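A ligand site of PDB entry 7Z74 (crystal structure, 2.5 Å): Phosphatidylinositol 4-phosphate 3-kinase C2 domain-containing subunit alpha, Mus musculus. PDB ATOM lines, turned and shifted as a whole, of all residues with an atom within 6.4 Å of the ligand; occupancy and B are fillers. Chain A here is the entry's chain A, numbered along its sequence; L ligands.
Merely in contact with the ligand: Ser 623 (2.9 Å), Glu 695 (3.0 Å), Ser 700 (3.0 Å), Met 646 (3.4 Å), Pro 698 (3.5 Å), Phe 682 (3.5 Å), Asn 644 (3.7 Å), Phe 622 (3.7 Å), Lys 630 (3.7 Å), Ile 777 (3.7 Å), Ala 699 (3.8 Å), Ser 624 (3.8 Å), Met 767 (3.8 Å) and Val 694 (3.96 Å).
Hydrophobic or aromatic side chains that line the ligand: Phe 622, Met 646, Phe 682, Val 694, Leu 696, Val 697, Pro 698, Met 767 and Ile 777.
16 residues have an atom within 4 Å of the ligand: Phe 622, Ser 623, Ser 624, Lys 630, Asn 644, Met 646, Phe 682, Val 694, Glu 695, Leu 696, Val 697, Pro 698, Ala 699, Ser 700, Met 767 and Ile 777.
The backbone carbonyl oxygen (O) of Arg 683 sits at hydrogen-bond distance from the backbone NH (N) of Glu 695, at 2.7 Å.
The side-chain hydroxyl of Ser 700 sits at hydrogen-bond distance from the backbone carbonyl oxygen of Val 697, 2.8 Å away.
The backbone carbonyl oxygen (O) of Met 646 sits at hydrogen-bond distance from the backbone NH (N) of Val 694.
The side-chain carboxylate (OE2) of Glu 642 lies within hydrogen-bond range of the side-chain amide nitrogen (ND2) of Asn 644.
The side-chain hydroxyl (OG1) of Thr 632 sits at hydrogen-bond distance from the side-chain amide oxygen (OD1) of Asn 644.
The backbone carbonyl oxygen of Pro 628 is in hydrogen-bond range of the backbone NH of Phe 622 (3.0 Å).
The side-chain hydroxyl (OG1) of Thr 632 is in hydrogen-bond range of the side-chain amino group (NZ) of Lys 630 (2.9 Å).
The backbone NH (N) of Phe 775 is in hydrogen-bond range of the backbone carbonyl oxygen (O) of Met 767, at 2.9 Å.
The backbone NH (N) of Val 697 lies within hydrogen-bond range of a nitrogen (N2) of the ligand.
The backbone carbonyl oxygen (O) of Val 697 sits at hydrogen-bond distance from a nitrogen (N5) of the ligand (3.2 Å).
The backbone carbonyl oxygen (O) of Leu 696 sits close to an oxygen (O3) of the ligand, at 3.3 Å.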
ATOM      1  N   PHE A 622     -31.160   0.305  26.555  1.00  0.00           N
ATOM      2  CA  PHE A 622     -30.884  -0.720  27.583  1.00  0.00           C
ATOM      3  C   PHE A 622     -32.191  -1.004  28.322  1.00  0.00           C
ATOM      4  O   PHE A 622     -33.015  -0.076  28.456  1.00  0.00           O
ATOM      5  CB  PHE A 622     -29.774  -0.258  28.531  1.00  0.00           C
ATOM      6  CG  PHE A 622     -28.428  -0.022  27.885  1.00  0.00           C
ATOM      7  CD1 PHE A 622     -27.493  -1.048  27.816  1.00  0.00           C
ATOM      8  CD2 PHE A 622     -28.094   1.205  27.350  1.00  0.00           C
ATOM      9  CE1 PHE A 622     -26.257  -0.836  27.223  1.00  0.00           C
ATOM     10  CE2 PHE A 622     -26.858   1.417  26.758  1.00  0.00           C
ATOM     11  CZ  PHE A 622     -25.948   0.395  26.705  1.00  0.00           C
ATOM     12  N   SER A 623     -32.398  -2.230  28.797  1.00  0.00           N
ATOM     13  CA  SER A 623     -33.627  -2.530  29.583  1.00  0.00           C
ATOM     14  C   SER A 623     -33.342  -2.369  31.072  1.00  0.00           C
ATOM     15  O   SER A 623     -32.597  -3.202  31.616  1.00  0.00           O
ATOM     16  CB  SER A 623     -34.158  -3.898  29.263  1.00  0.00           C
ATOM     17  OG  SER A 623     -35.353  -4.151  29.980  1.00  0.00           O
ATOM     18  N   SER A 624     -33.933  -1.359  31.702  1.00  0.00           N
ATOM     19  CA  SER A 624     -33.673  -1.071  33.137  1.00  0.00           C
ATOM     20  C   SER A 624     -34.818  -0.216  33.689  1.00  0.00           C
ATOM     21  O   SER A 624     -35.725   0.114  32.915  1.00  0.00           O
ATOM     22  CB  SER A 624     -32.335  -0.436  33.347  1.00  0.00           C
ATOM     23  OG  SER A 624     -32.222   0.757  32.593  1.00  0.00           O
ATOM     24  N   PRO A 628     -32.355   3.615  29.359  1.00  0.00           N
ATOM     25  CA  PRO A 628     -31.354   4.515  28.816  1.00  0.00           C
ATOM     26  C   PRO A 628     -31.246   4.315  27.303  1.00  0.00           C
ATOM     27  O   PRO A 628     -31.638   3.272  26.820  1.00  0.00           O
ATOM     28  CB  PRO A 628     -30.059   4.099  29.510  1.00  0.00           C
ATOM     29  CG  PRO A 628     -30.457   3.013  30.490  1.00  0.00           C
ATOM     30  CD  PRO A 628     -31.723   2.425  29.927  1.00  0.00           C
ATOM     31  N   LYS A 630     -28.909   3.814  24.021  1.00  0.00           N
ATOM     32  CA  LYS A 630     -27.540   3.532  23.517  1.00  0.00           C
ATOM     33  C   LYS A 630     -27.395   4.332  22.225  1.00  0.00           C
ATOM     34  O   LYS A 630     -27.976   3.924  21.212  1.00  0.00           O
ATOM     35  CB  LYS A 630     -27.314   2.046  23.260  1.00  0.00           C
ATOM     36  CG  LYS A 630     -25.959   1.684  22.670  1.00  0.00           C
ATOM     37  CD  LYS A 630     -25.802   0.214  22.357  1.00  0.00           C
ATOM     38  CE  LYS A 630     -24.504  -0.101  21.648  1.00  0.00           C
ATOM     39  NZ  LYS A 630     -24.426   0.573  20.324  1.00  0.00           N
ATOM     40  N   THR A 632     -25.201   5.617  19.228  1.00  0.00           N
ATOM     41  CA  THR A 632     -23.996   5.407  18.442  1.00  0.00           C
ATOM     42  C   THR A 632     -23.960   6.433  17.316  1.00  0.00           C
ATOM     43  O   THR A 632     -24.920   6.553  16.550  1.00  0.00           O
ATOM     44  CB  THR A 632     -23.945   3.998  17.841  1.00  0.00           C
ATOM     45  OG1 THR A 632     -24.235   3.037  18.860  1.00  0.00           O
ATOM     46  CG2 THR A 632     -22.560   3.726  17.286  1.00  0.00           C
ATOM     47  N   GLU A 641     -12.555   6.226  15.876  1.00  0.00           N
ATOM     48  CA  GLU A 641     -13.529   5.164  16.107  1.00  0.00           C
ATOM     49  C   GLU A 641     -14.920   5.762  16.226  1.00  0.00           C
ATOM     50  O   GLU A 641     -15.097   6.982  16.365  1.00  0.00           O
ATOM     51  CB  GLU A 641     -13.167   4.384  17.384  1.00  0.00           C
ATOM     52  CG  GLU A 641     -11.699   3.995  17.520  1.00  0.00           C
ATOM     53  CD  GLU A 641     -11.108   3.466  16.224  1.00  0.00           C
ATOM     54  OE1 GLU A 641     -10.007   3.935  15.832  1.00  0.00           O
ATOM     55  OE2 GLU A 641     -11.746   2.579  15.595  1.00  0.00           O
ATOM     56  N   GLU A 642     -15.923   4.901  16.184  1.00  0.00           N
ATOM     57  CA  GLU A 642     -17.283   5.387  16.327  1.00  0.00           C
ATOM     58  C   GLU A 642     -17.576   5.688  17.797  1.00  0.00           C
ATOM     59  O   GLU A 642     -16.983   5.113  18.714  1.00  0.00           O
ATOM     60  CB  GLU A 642     -18.284   4.385  15.759  1.00  0.00           C
ATOM     61  CG  GLU A 642     -18.431   3.122  16.570  1.00  0.00           C
ATOM     62  CD  GLU A 642     -19.641   2.310  16.170  1.00  0.00           C
ATOM     63  OE1 GLU A 642     -20.269   2.618  15.120  1.00  0.00           O
ATOM     64  OE2 GLU A 642     -19.984   1.369  16.924  1.00  0.00           O
ATOM     65  N   ILE A 643     -18.492   6.625  18.002  1.00  0.00           N
ATOM     66  CA  ILE A 643     -18.760   7.227  19.301  1.00  0.00           C
ATOM     67  C   ILE A 643     -19.953   6.526  19.916  1.00  0.00           C
ATOM     68  O   ILE A 643     -20.991   6.357  19.257  1.00  0.00           O
ATOM     69  CB  ILE A 643     -19.013   8.735  19.155  1.00  0.00           C
ATOM     70  CG1 ILE A 643     -17.857   9.392  18.383  1.00  0.00           C
ATOM     71  CG2 ILE A 643     -19.222   9.388  20.528  1.00  0.00           C
ATOM     72  CD1 ILE A 643     -18.241  10.668  17.681  1.00  0.00           C
ATOM     73  N   ASN A 644     -19.823   6.111  21.174  1.00  0.00           N
ATOM     74  CA  ASN A 644     -20.873   5.375  21.870  1.00  0.00           C
ATOM     75  C   ASN A 644     -21.094   6.006  23.230  1.00  0.00           C
ATOM     76  O   ASN A 644     -20.180   6.030  24.057  1.00  0.00           O
ATOM     77  CB  ASN A 644     -20.504   3.903  22.016  1.00  0.00           C
ATOM     78  CG  ASN A 644     -20.769   3.111  20.756  1.00  0.00           C
ATOM     79  OD1 ASN A 644     -21.921   2.814  20.442  1.00  0.00           O
ATOM     80  ND2 ASN A 644     -19.709   2.802  20.013  1.00  0.00           N
ATOM     81  N   VAL A 645     -22.304   6.532  23.459  1.00  0.00           N
ATOM     82  CA  VAL A 645     -22.644   7.110  24.759  1.00  0.00           C
ATOM     83  C   VAL A 645     -24.001   6.577  25.177  1.00  0.00           C
ATOM     84  O   VAL A 645     -24.800   6.105  24.373  1.00  0.00           O
ATOM     85  CB  VAL A 645     -22.685   8.647  24.750  1.00  0.00           C
ATOM     86  CG1 VAL A 645     -21.386   9.200  24.181  1.00  0.00           C
ATOM     87  CG2 VAL A 645     -23.908   9.159  23.978  1.00  0.00           C
ATOM     88  N   MET A 646     -24.251   6.650  26.481  1.00  0.00           N
ATOM     89  CA  MET A 646     -25.567   6.359  26.989  1.00  0.00           C
ATOM     90  C   MET A 646     -26.221   7.679  27.347  1.00  0.00           C
ATOM     91  O   MET A 646     -25.561   8.595  27.858  1.00  0.00           O
ATOM     92  CB  MET A 646     -25.489   5.436  28.204  1.00  0.00           C
ATOM     93  CG  MET A 646     -26.696   5.513  29.114  1.00  0.00           C
ATOM     94  SD  MET A 646     -26.464   4.634  30.670  1.00  0.00           S
ATOM     95  CE  MET A 646     -26.593   2.920  30.143  1.00  0.00           C
ATOM     96  N   LYS A 648     -29.406   9.042  29.580  1.00  0.00           N
ATOM     97  CA  LYS A 648     -30.353   8.637  30.594  1.00  0.00           C
ATOM     98  C   LYS A 648     -31.182   9.846  30.997  1.00  0.00           C
ATOM     99  O   LYS A 648     -30.636  10.937  31.187  1.00  0.00           O
ATOM    100  CB  LYS A 648     -29.616   8.057  31.821  1.00  0.00           C
ATOM    101  CG  LYS A 648     -30.418   7.079  32.654  1.00  0.00           C
ATOM    102  CD  LYS A 648     -29.702   6.740  33.972  1.00  0.00           C
ATOM    103  CE  LYS A 648     -28.308   6.152  33.754  1.00  0.00           C
ATOM    104  NZ  LYS A 648     -27.394   6.356  34.945  1.00  0.00           N
ATOM    105  N   PHE A 682     -14.579   6.426  34.296  1.00  0.00           N
ATOM    106  CA  PHE A 682     -15.466   6.816  33.211  1.00  0.00           C
ATOM    107  C   PHE A 682     -16.270   8.059  33.563  1.00  0.00           C
ATOM    108  O   PHE A 682     -16.585   8.356  34.715  1.00  0.00           O
ATOM    109  CB  PHE A 682     -16.397   5.654  32.806  1.00  0.00           C
ATOM    110  CG  PHE A 682     -17.463   5.324  33.802  1.00  0.00           C
ATOM    111  CD1 PHE A 682     -18.683   5.985  33.775  1.00  0.00           C
ATOM    112  CD2 PHE A 682     -17.282   4.298  34.721  1.00  0.00           C
ATOM    113  CE1 PHE A 682     -19.676   5.664  34.684  1.00  0.00           C
ATOM    114  CE2 PHE A 682     -18.295   3.966  35.621  1.00  0.00           C
ATOM    115  CZ  PHE A 682     -19.488   4.644  35.601  1.00  0.00           C
ATOM    116  N   ARG A 683     -16.575   8.792  32.488  1.00  0.00           N
ATOM    117  CA  ARG A 683     -17.343  10.028  32.442  1.00  0.00           C
ATOM    118  C   ARG A 683     -18.863   9.939  32.574  1.00  0.00           C
ATOM    119  O   ARG A 683     -19.515   9.029  32.062  1.00  0.00           O
ATOM    120  CB  ARG A 683     -17.008  10.694  31.122  1.00  0.00           C
ATOM    121  CG  ARG A 683     -15.742  11.462  31.136  1.00  0.00           C
ATOM    122  CD  ARG A 683     -15.266  11.863  29.749  1.00  0.00           C
ATOM    123  NE  ARG A 683     -14.219  12.879  29.873  1.00  0.00           N
ATOM    124  CZ  ARG A 683     -13.350  13.291  28.971  1.00  0.00           C
ATOM    125  NH1 ARG A 683     -13.033  12.479  27.989  1.00  0.00           N
ATOM    126  NH2 ARG A 683     -12.595  14.363  29.197  1.00  0.00           N
ATOM    127  N   VAL A 694     -23.707   9.474  29.865  1.00  0.00           N
ATOM    128  CA  VAL A 694     -22.752   8.661  30.600  1.00  0.00           C
ATOM    129  C   VAL A 694     -21.868   7.934  29.588  1.00  0.00           C
ATOM    130  O   VAL A 694     -22.332   7.509  28.524  1.00  0.00           O
ATOM    131  CB  VAL A 694     -23.477   7.652  31.523  1.00  0.00           C
ATOM    132  CG1 VAL A 694     -22.508   7.023  32.504  1.00  0.00           C
ATOM    133  CG2 VAL A 694     -24.611   8.327  32.251  1.00  0.00           C
ATOM    134  N   GLU A 695     -20.585   7.796  29.920  1.00  0.00           N
ATOM    135  CA  GLU A 695     -19.681   7.003  29.113  1.00  0.00           C
ATOM    136  C   GLU A 695     -20.058   5.526  29.165  1.00  0.00           C
ATOM    137  O   GLU A 695     -20.506   5.014  30.201  1.00  0.00           O
ATOM    138  CB  GLU A 695     -18.238   7.195  29.598  1.00  0.00           C
ATOM    139  CG  GLU A 695     -17.177   6.438  28.799  1.00  0.00           C
ATOM    140  CD  GLU A 695     -15.766   6.714  29.311  1.00  0.00           C
ATOM    141  OE1 GLU A 695     -15.580   7.732  30.017  1.00  0.00           O
ATOM    142  OE2 GLU A 695     -14.864   5.915  28.987  1.00  0.00           O
ATOM    143  N   LEU A 696     -19.900   4.843  28.034  1.00  0.00           N
ATOM    144  CA  LEU A 696     -20.063   3.393  27.944  1.00  0.00           C
ATOM    145  C   LEU A 696     -18.690   2.736  27.962  1.00  0.00           C
ATOM    146  O   LEU A 696     -17.797   3.121  27.207  1.00  0.00           O
ATOM    147  CB  LEU A 696     -20.827   3.008  26.675  1.00  0.00           C
ATOM    148  CG  LEU A 696     -22.320   3.328  26.715  1.00  0.00           C
ATOM    149  CD1 LEU A 696     -23.000   2.958  25.417  1.00  0.00           C
ATOM    150  CD2 LEU A 696     -22.973   2.609  27.881  1.00  0.00           C
ATOM    151  N   VAL A 697     -18.531   1.754  28.840  1.00  0.00           N
ATOM    152  CA  VAL A 697     -17.289   0.981  28.947  1.00  0.00           C
ATOM    153  C   VAL A 697     -17.434  -0.244  28.041  1.00  0.00           C
ATOM    154  O   VAL A 697     -18.356  -1.043  28.270  1.00  0.00           O
ATOM    155  CB  VAL A 697     -16.999   0.578  30.390  1.00  0.00           C
ATOM    156  CG1 VAL A 697     -15.697  -0.162  30.478  1.00  0.00           C
ATOM    157  CG2 VAL A 697     -16.966   1.804  31.276  1.00  0.00           C
ATOM    158  N   PRO A 698     -16.604  -0.414  27.024  1.00  0.00           N
ATOM    159  CA  PRO A 698     -16.832  -1.502  26.070  1.00  0.00           C
ATOM    160  C   PRO A 698     -16.473  -2.849  26.669  1.00  0.00           C
ATOM    161  O   PRO A 698     -15.577  -2.960  27.513  1.00  0.00           O
ATOM    162  CB  PRO A 698     -15.901  -1.146  24.907  1.00  0.00           C
ATOM    163  CG  PRO A 698     -14.799  -0.423  25.550  1.00  0.00           C
ATOM    164  CD  PRO A 698     -15.428   0.384  26.666  1.00  0.00           C
ATOM    165  N   ALA A 699     -17.203  -3.865  26.228  1.00  0.00           N
ATOM    166  CA  ALA A 699     -16.940  -5.269  26.561  1.00  0.00           C
ATOM    167  C   ALA A 699     -16.862  -5.466  28.069  1.00  0.00           C
ATOM    168  O   ALA A 699     -15.830  -5.850  28.627  1.00  0.00           O
ATOM    169  CB  ALA A 699     -15.673  -5.789  25.860  1.00  0.00           C
ATOM    170  N   SER A 700     -17.985  -5.207  28.725  1.00  0.00           N
ATOM    171  CA  SER A 700     -18.089  -5.365  30.166  1.00  0.00           C
ATOM    172  C   SER A 700     -19.527  -5.724  30.516  1.00  0.00           C
ATOM    173  O   SER A 700     -20.462  -5.314  29.820  1.00  0.00           O
ATOM    174  CB  SER A 700     -17.690  -4.079  30.896  1.00  0.00           C
ATOM    175  OG  SER A 700     -18.349  -2.970  30.323  1.00  0.00           O
ATOM    176  N   ASP A 701     -19.680  -6.496  31.579  1.00  0.00           N
ATOM    177  CA  ASP A 701     -21.001  -6.928  32.039  1.00  0.00           C
ATOM    178  C   ASP A 701     -21.101  -6.820  33.549  1.00  0.00           C
ATOM    179  O   ASP A 701     -20.102  -6.795  34.262  1.00  0.00           O
ATOM    180  CB  ASP A 701     -21.334  -8.370  31.611  1.00  0.00           C
ATOM    181  CG  ASP A 701     -22.050  -8.425  30.287  1.00  0.00           C
ATOM    182  OD1 ASP A 701     -21.653  -9.247  29.419  1.00  0.00           O
ATOM    183  OD2 ASP A 701     -23.039  -7.674  30.132  1.00  0.00           O
ATOM    184  N   THR A 702     -22.336  -6.782  34.020  1.00  0.00           N
ATOM    185  CA  THR A 702     -22.593  -6.905  35.437  1.00  0.00           C
ATOM    186  C   THR A 702     -22.310  -8.338  35.897  1.00  0.00           C
ATOM    187  O   THR A 702     -22.296  -9.290  35.118  1.00  0.00           O
ATOM    188  CB  THR A 702     -24.030  -6.520  35.765  1.00  0.00           C
ATOM    189  OG1 THR A 702     -24.925  -7.528  35.278  1.00  0.00           O
ATOM    190  CG2 THR A 702     -24.374  -5.191  35.121  1.00  0.00           C
ATOM    191  N   ASP A 764     -25.711  -6.281  40.098  1.00  0.00           N
ATOM    192  CA  ASP A 764     -25.937  -5.269  39.028  1.00  0.00           C
ATOM    193  C   ASP A 764     -24.966  -4.100  39.178  1.00  0.00           C
ATOM    194  O   ASP A 764     -24.338  -3.734  38.178  1.00  0.00           O
ATOM    195  CB  ASP A 764     -27.392  -4.813  38.984  1.00  0.00           C
ATOM    196  CG  ASP A 764     -28.341  -5.853  38.400  1.00  0.00           C
ATOM    197  OD1 ASP A 764     -27.949  -6.501  37.407  1.00  0.00           O
ATOM    198  OD2 ASP A 764     -29.446  -6.001  38.944  1.00  0.00           O
ATOM    199  N   MET A 767     -19.633  -4.015  37.903  1.00  0.00           N
ATOM    200  CA  MET A 767     -19.379  -4.413  36.530  1.00  0.00           C
ATOM    201  C   MET A 767     -17.927  -4.813  36.354  1.00  0.00           C
ATOM    202  O   MET A 767     -17.013  -4.279  37.002  1.00  0.00           O
ATOM    203  CB  MET A 767     -19.734  -3.307  35.545  1.00  0.00           C
ATOM    204  CG  MET A 767     -21.230  -3.162  35.359  1.00  0.00           C
ATOM    205  SD  MET A 767     -21.705  -2.200  33.921  1.00  0.00           S
ATOM    206  CE  MET A 767     -20.568  -2.827  32.698  1.00  0.00           C
ATOM    207  N   PHE A 775     -15.249  -2.322  38.228  1.00  0.00           N
ATOM    208  CA  PHE A 775     -15.685  -0.949  38.489  1.00  0.00           C
ATOM    209  C   PHE A 775     -17.144  -0.955  38.970  1.00  0.00           C
ATOM    210  O   PHE A 775     -17.811  -1.990  38.972  1.00  0.00           O
ATOM    211  CB  PHE A 775     -15.490  -0.048  37.242  1.00  0.00           C
ATOM    212  CG  PHE A 775     -16.202  -0.540  35.997  1.00  0.00           C
ATOM    213  CD1 PHE A 775     -15.673  -1.556  35.230  1.00  0.00           C
ATOM    214  CD2 PHE A 775     -17.388   0.054  35.582  1.00  0.00           C
ATOM    215  CE1 PHE A 775     -16.325  -1.999  34.096  1.00  0.00           C
ATOM    216  CE2 PHE A 775     -18.039  -0.377  34.442  1.00  0.00           C
ATOM    217  CZ  PHE A 775     -17.507  -1.407  33.694  1.00  0.00           C
ATOM    218  N   HIS A 776     -17.611   0.222  39.398  1.00  0.00           N
ATOM    219  CA  HIS A 776     -18.965   0.435  39.899  1.00  0.00           C
ATOM    220  C   HIS A 776     -19.721   1.348  38.943  1.00  0.00           C
ATOM    221  O   HIS A 776     -19.111   2.237  38.337  1.00  0.00           O
ATOM    222  CB  HIS A 776     -18.947   1.090  41.288  1.00  0.00           C
ATOM    223  CG  HIS A 776     -18.250   0.283  42.335  1.00  0.00           C
ATOM    224  ND1 HIS A 776     -18.552  -1.038  42.579  1.00  0.00           N
ATOM    225  CD2 HIS A 776     -17.253   0.607  43.190  1.00  0.00           C
ATOM    226  CE1 HIS A 776     -17.772  -1.486  43.539  1.00  0.00           C
ATOM    227  NE2 HIS A 776     -16.976  -0.505  43.931  1.00  0.00           N
ATOM    228  N   ILE A 777     -21.044   1.169  38.823  1.00  0.00           N
ATOM    229  CA  ILE A 777     -21.838   1.978  37.908  1.00  0.00           C
ATOM    230  C   ILE A 777     -22.952   2.750  38.608  1.00  0.00           C
ATOM    231  O   ILE A 777     -23.162   3.928  38.332  1.00  0.00           O
ATOM    232  CB  ILE A 777     -22.414   1.133  36.741  1.00  0.00           C
ATOM    233  CG1 ILE A 777     -23.217  -0.075  37.251  1.00  0.00           C
ATOM    234  CG2 ILE A 777     -21.290   0.739  35.801  1.00  0.00           C
ATOM    235  CD1 ILE A 777     -24.341  -0.485  36.306  1.00  0.00           C
ATOM    236  N   ASP A 778     -23.686   2.102  39.507  1.00  0.00           N
ATOM    237  CA  ASP A 778     -24.804   2.792  40.148  1.00  0.00           C
ATOM    238  C   ASP A 778     -24.398   3.153  41.566  1.00  0.00           C
ATOM    239  O   ASP A 778     -23.928   2.297  42.321  1.00  0.00           O
ATOM    240  CB  ASP A 778     -26.074   1.953  40.151  1.00  0.00           C
ATOM    241  CG  ASP A 778     -26.688   1.800  38.774  1.00  0.00           C
ATOM    242  OD1 ASP A 778     -27.318   0.748  38.535  1.00  0.00           O
ATOM    243  OD2 ASP A 778     -26.536   2.727  37.960  1.00  0.00           O
HETATM  244  C1  LIG L   1     -21.476   3.219  32.928  1.00  0.00           C
HETATM  245  C2  LIG L   1     -24.018   0.828  31.896  1.00  0.00           C
HETATM  246  C3  LIG L   1     -25.589  -2.040  31.957  1.00  0.00           C
HETATM  247  C4  LIG L   1     -28.886  -3.539  30.835  1.00  0.00           C
HETATM  248  C5  LIG L   1     -29.700  -3.248  31.925  1.00  0.00           C
HETATM  249  C6  LIG L   1     -29.184  -2.582  33.023  1.00  0.00           C
HETATM  250  C7  LIG L   1     -18.567   1.004  23.456  1.00  0.00           C
HETATM  251  C8  LIG L   1     -21.200  -2.268  27.432  1.00  0.00           C
HETATM  252  C9  LIG L   1     -21.541  -2.655  28.870  1.00  0.00           C
HETATM  253  C10 LIG L   1     -23.076  -0.644  30.379  1.00  0.00           C
HETATM  254  C11 LIG L   1     -21.722   1.071  31.286  1.00  0.00           C
HETATM  255  C12 LIG L   1     -20.388   2.759  32.183  1.00  0.00           C
HETATM  256  C13 LIG L   1     -22.779   1.504  32.017  1.00  0.00           C
HETATM  257  C14 LIG L   1     -25.406  -0.882  30.979  1.00  0.00           C
HETATM  258  C15 LIG L   1     -27.042  -2.475  31.950  1.00  0.00           C
HETATM  259  C16 LIG L   1     -27.565  -3.147  30.855  1.00  0.00           C
HETATM  260  C17 LIG L   1     -27.854  -2.190  33.032  1.00  0.00           C
HETATM  261  C18 LIG L   1     -20.942  -0.486  25.662  1.00  0.00           C
HETATM  262  C19 LIG L   1     -19.698   0.388  23.974  1.00  0.00           C
HETATM  263  C20 LIG L   1     -17.945   0.524  22.313  1.00  0.00           C
HETATM  264  C21 LIG L   1     -16.811   1.160  21.819  1.00  0.00           C
HETATM  265  C22 LIG L   1     -16.291   2.270  22.473  1.00  0.00           C
HETATM  266  C23 LIG L   1     -16.900   2.754  23.628  1.00  0.00           C
HETATM  267  C24 LIG L   1     -18.039   2.119  24.108  1.00  0.00           C
HETATM  268  C25 LIG L   1     -20.784   0.047  23.172  1.00  0.00           C
HETATM  269  N1  LIG L   1     -21.886  -0.022  30.452  1.00  0.00           N
HETATM  270  N2  LIG L   1     -20.514   1.710  31.377  1.00  0.00           N
HETATM  271  N3  LIG L   1     -22.643   2.597  32.846  1.00  0.00           N
HETATM  272  N4  LIG L   1     -24.122  -0.215  31.090  1.00  0.00           N
HETATM  273  N5  LIG L   1     -21.264  -0.872  27.033  1.00  0.00           N
HETATM  274  N6  LIG L   1     -19.823   0.101  25.253  1.00  0.00           N
HETATM  275  O1  LIG L   1     -20.892  -3.123  26.661  1.00  0.00           O
HETATM  276  O2  LIG L   1     -24.950   1.201  32.531  1.00  0.00           O
HETATM  277  O3  LIG L   1     -16.380   3.880  24.284  1.00  0.00           O
HETATM  278  S1  LIG L   1     -23.219  -2.075  29.265  1.00  0.00           S
HETATM  279  S2  LIG L   1     -21.933  -0.670  24.260  1.00  0.00           S
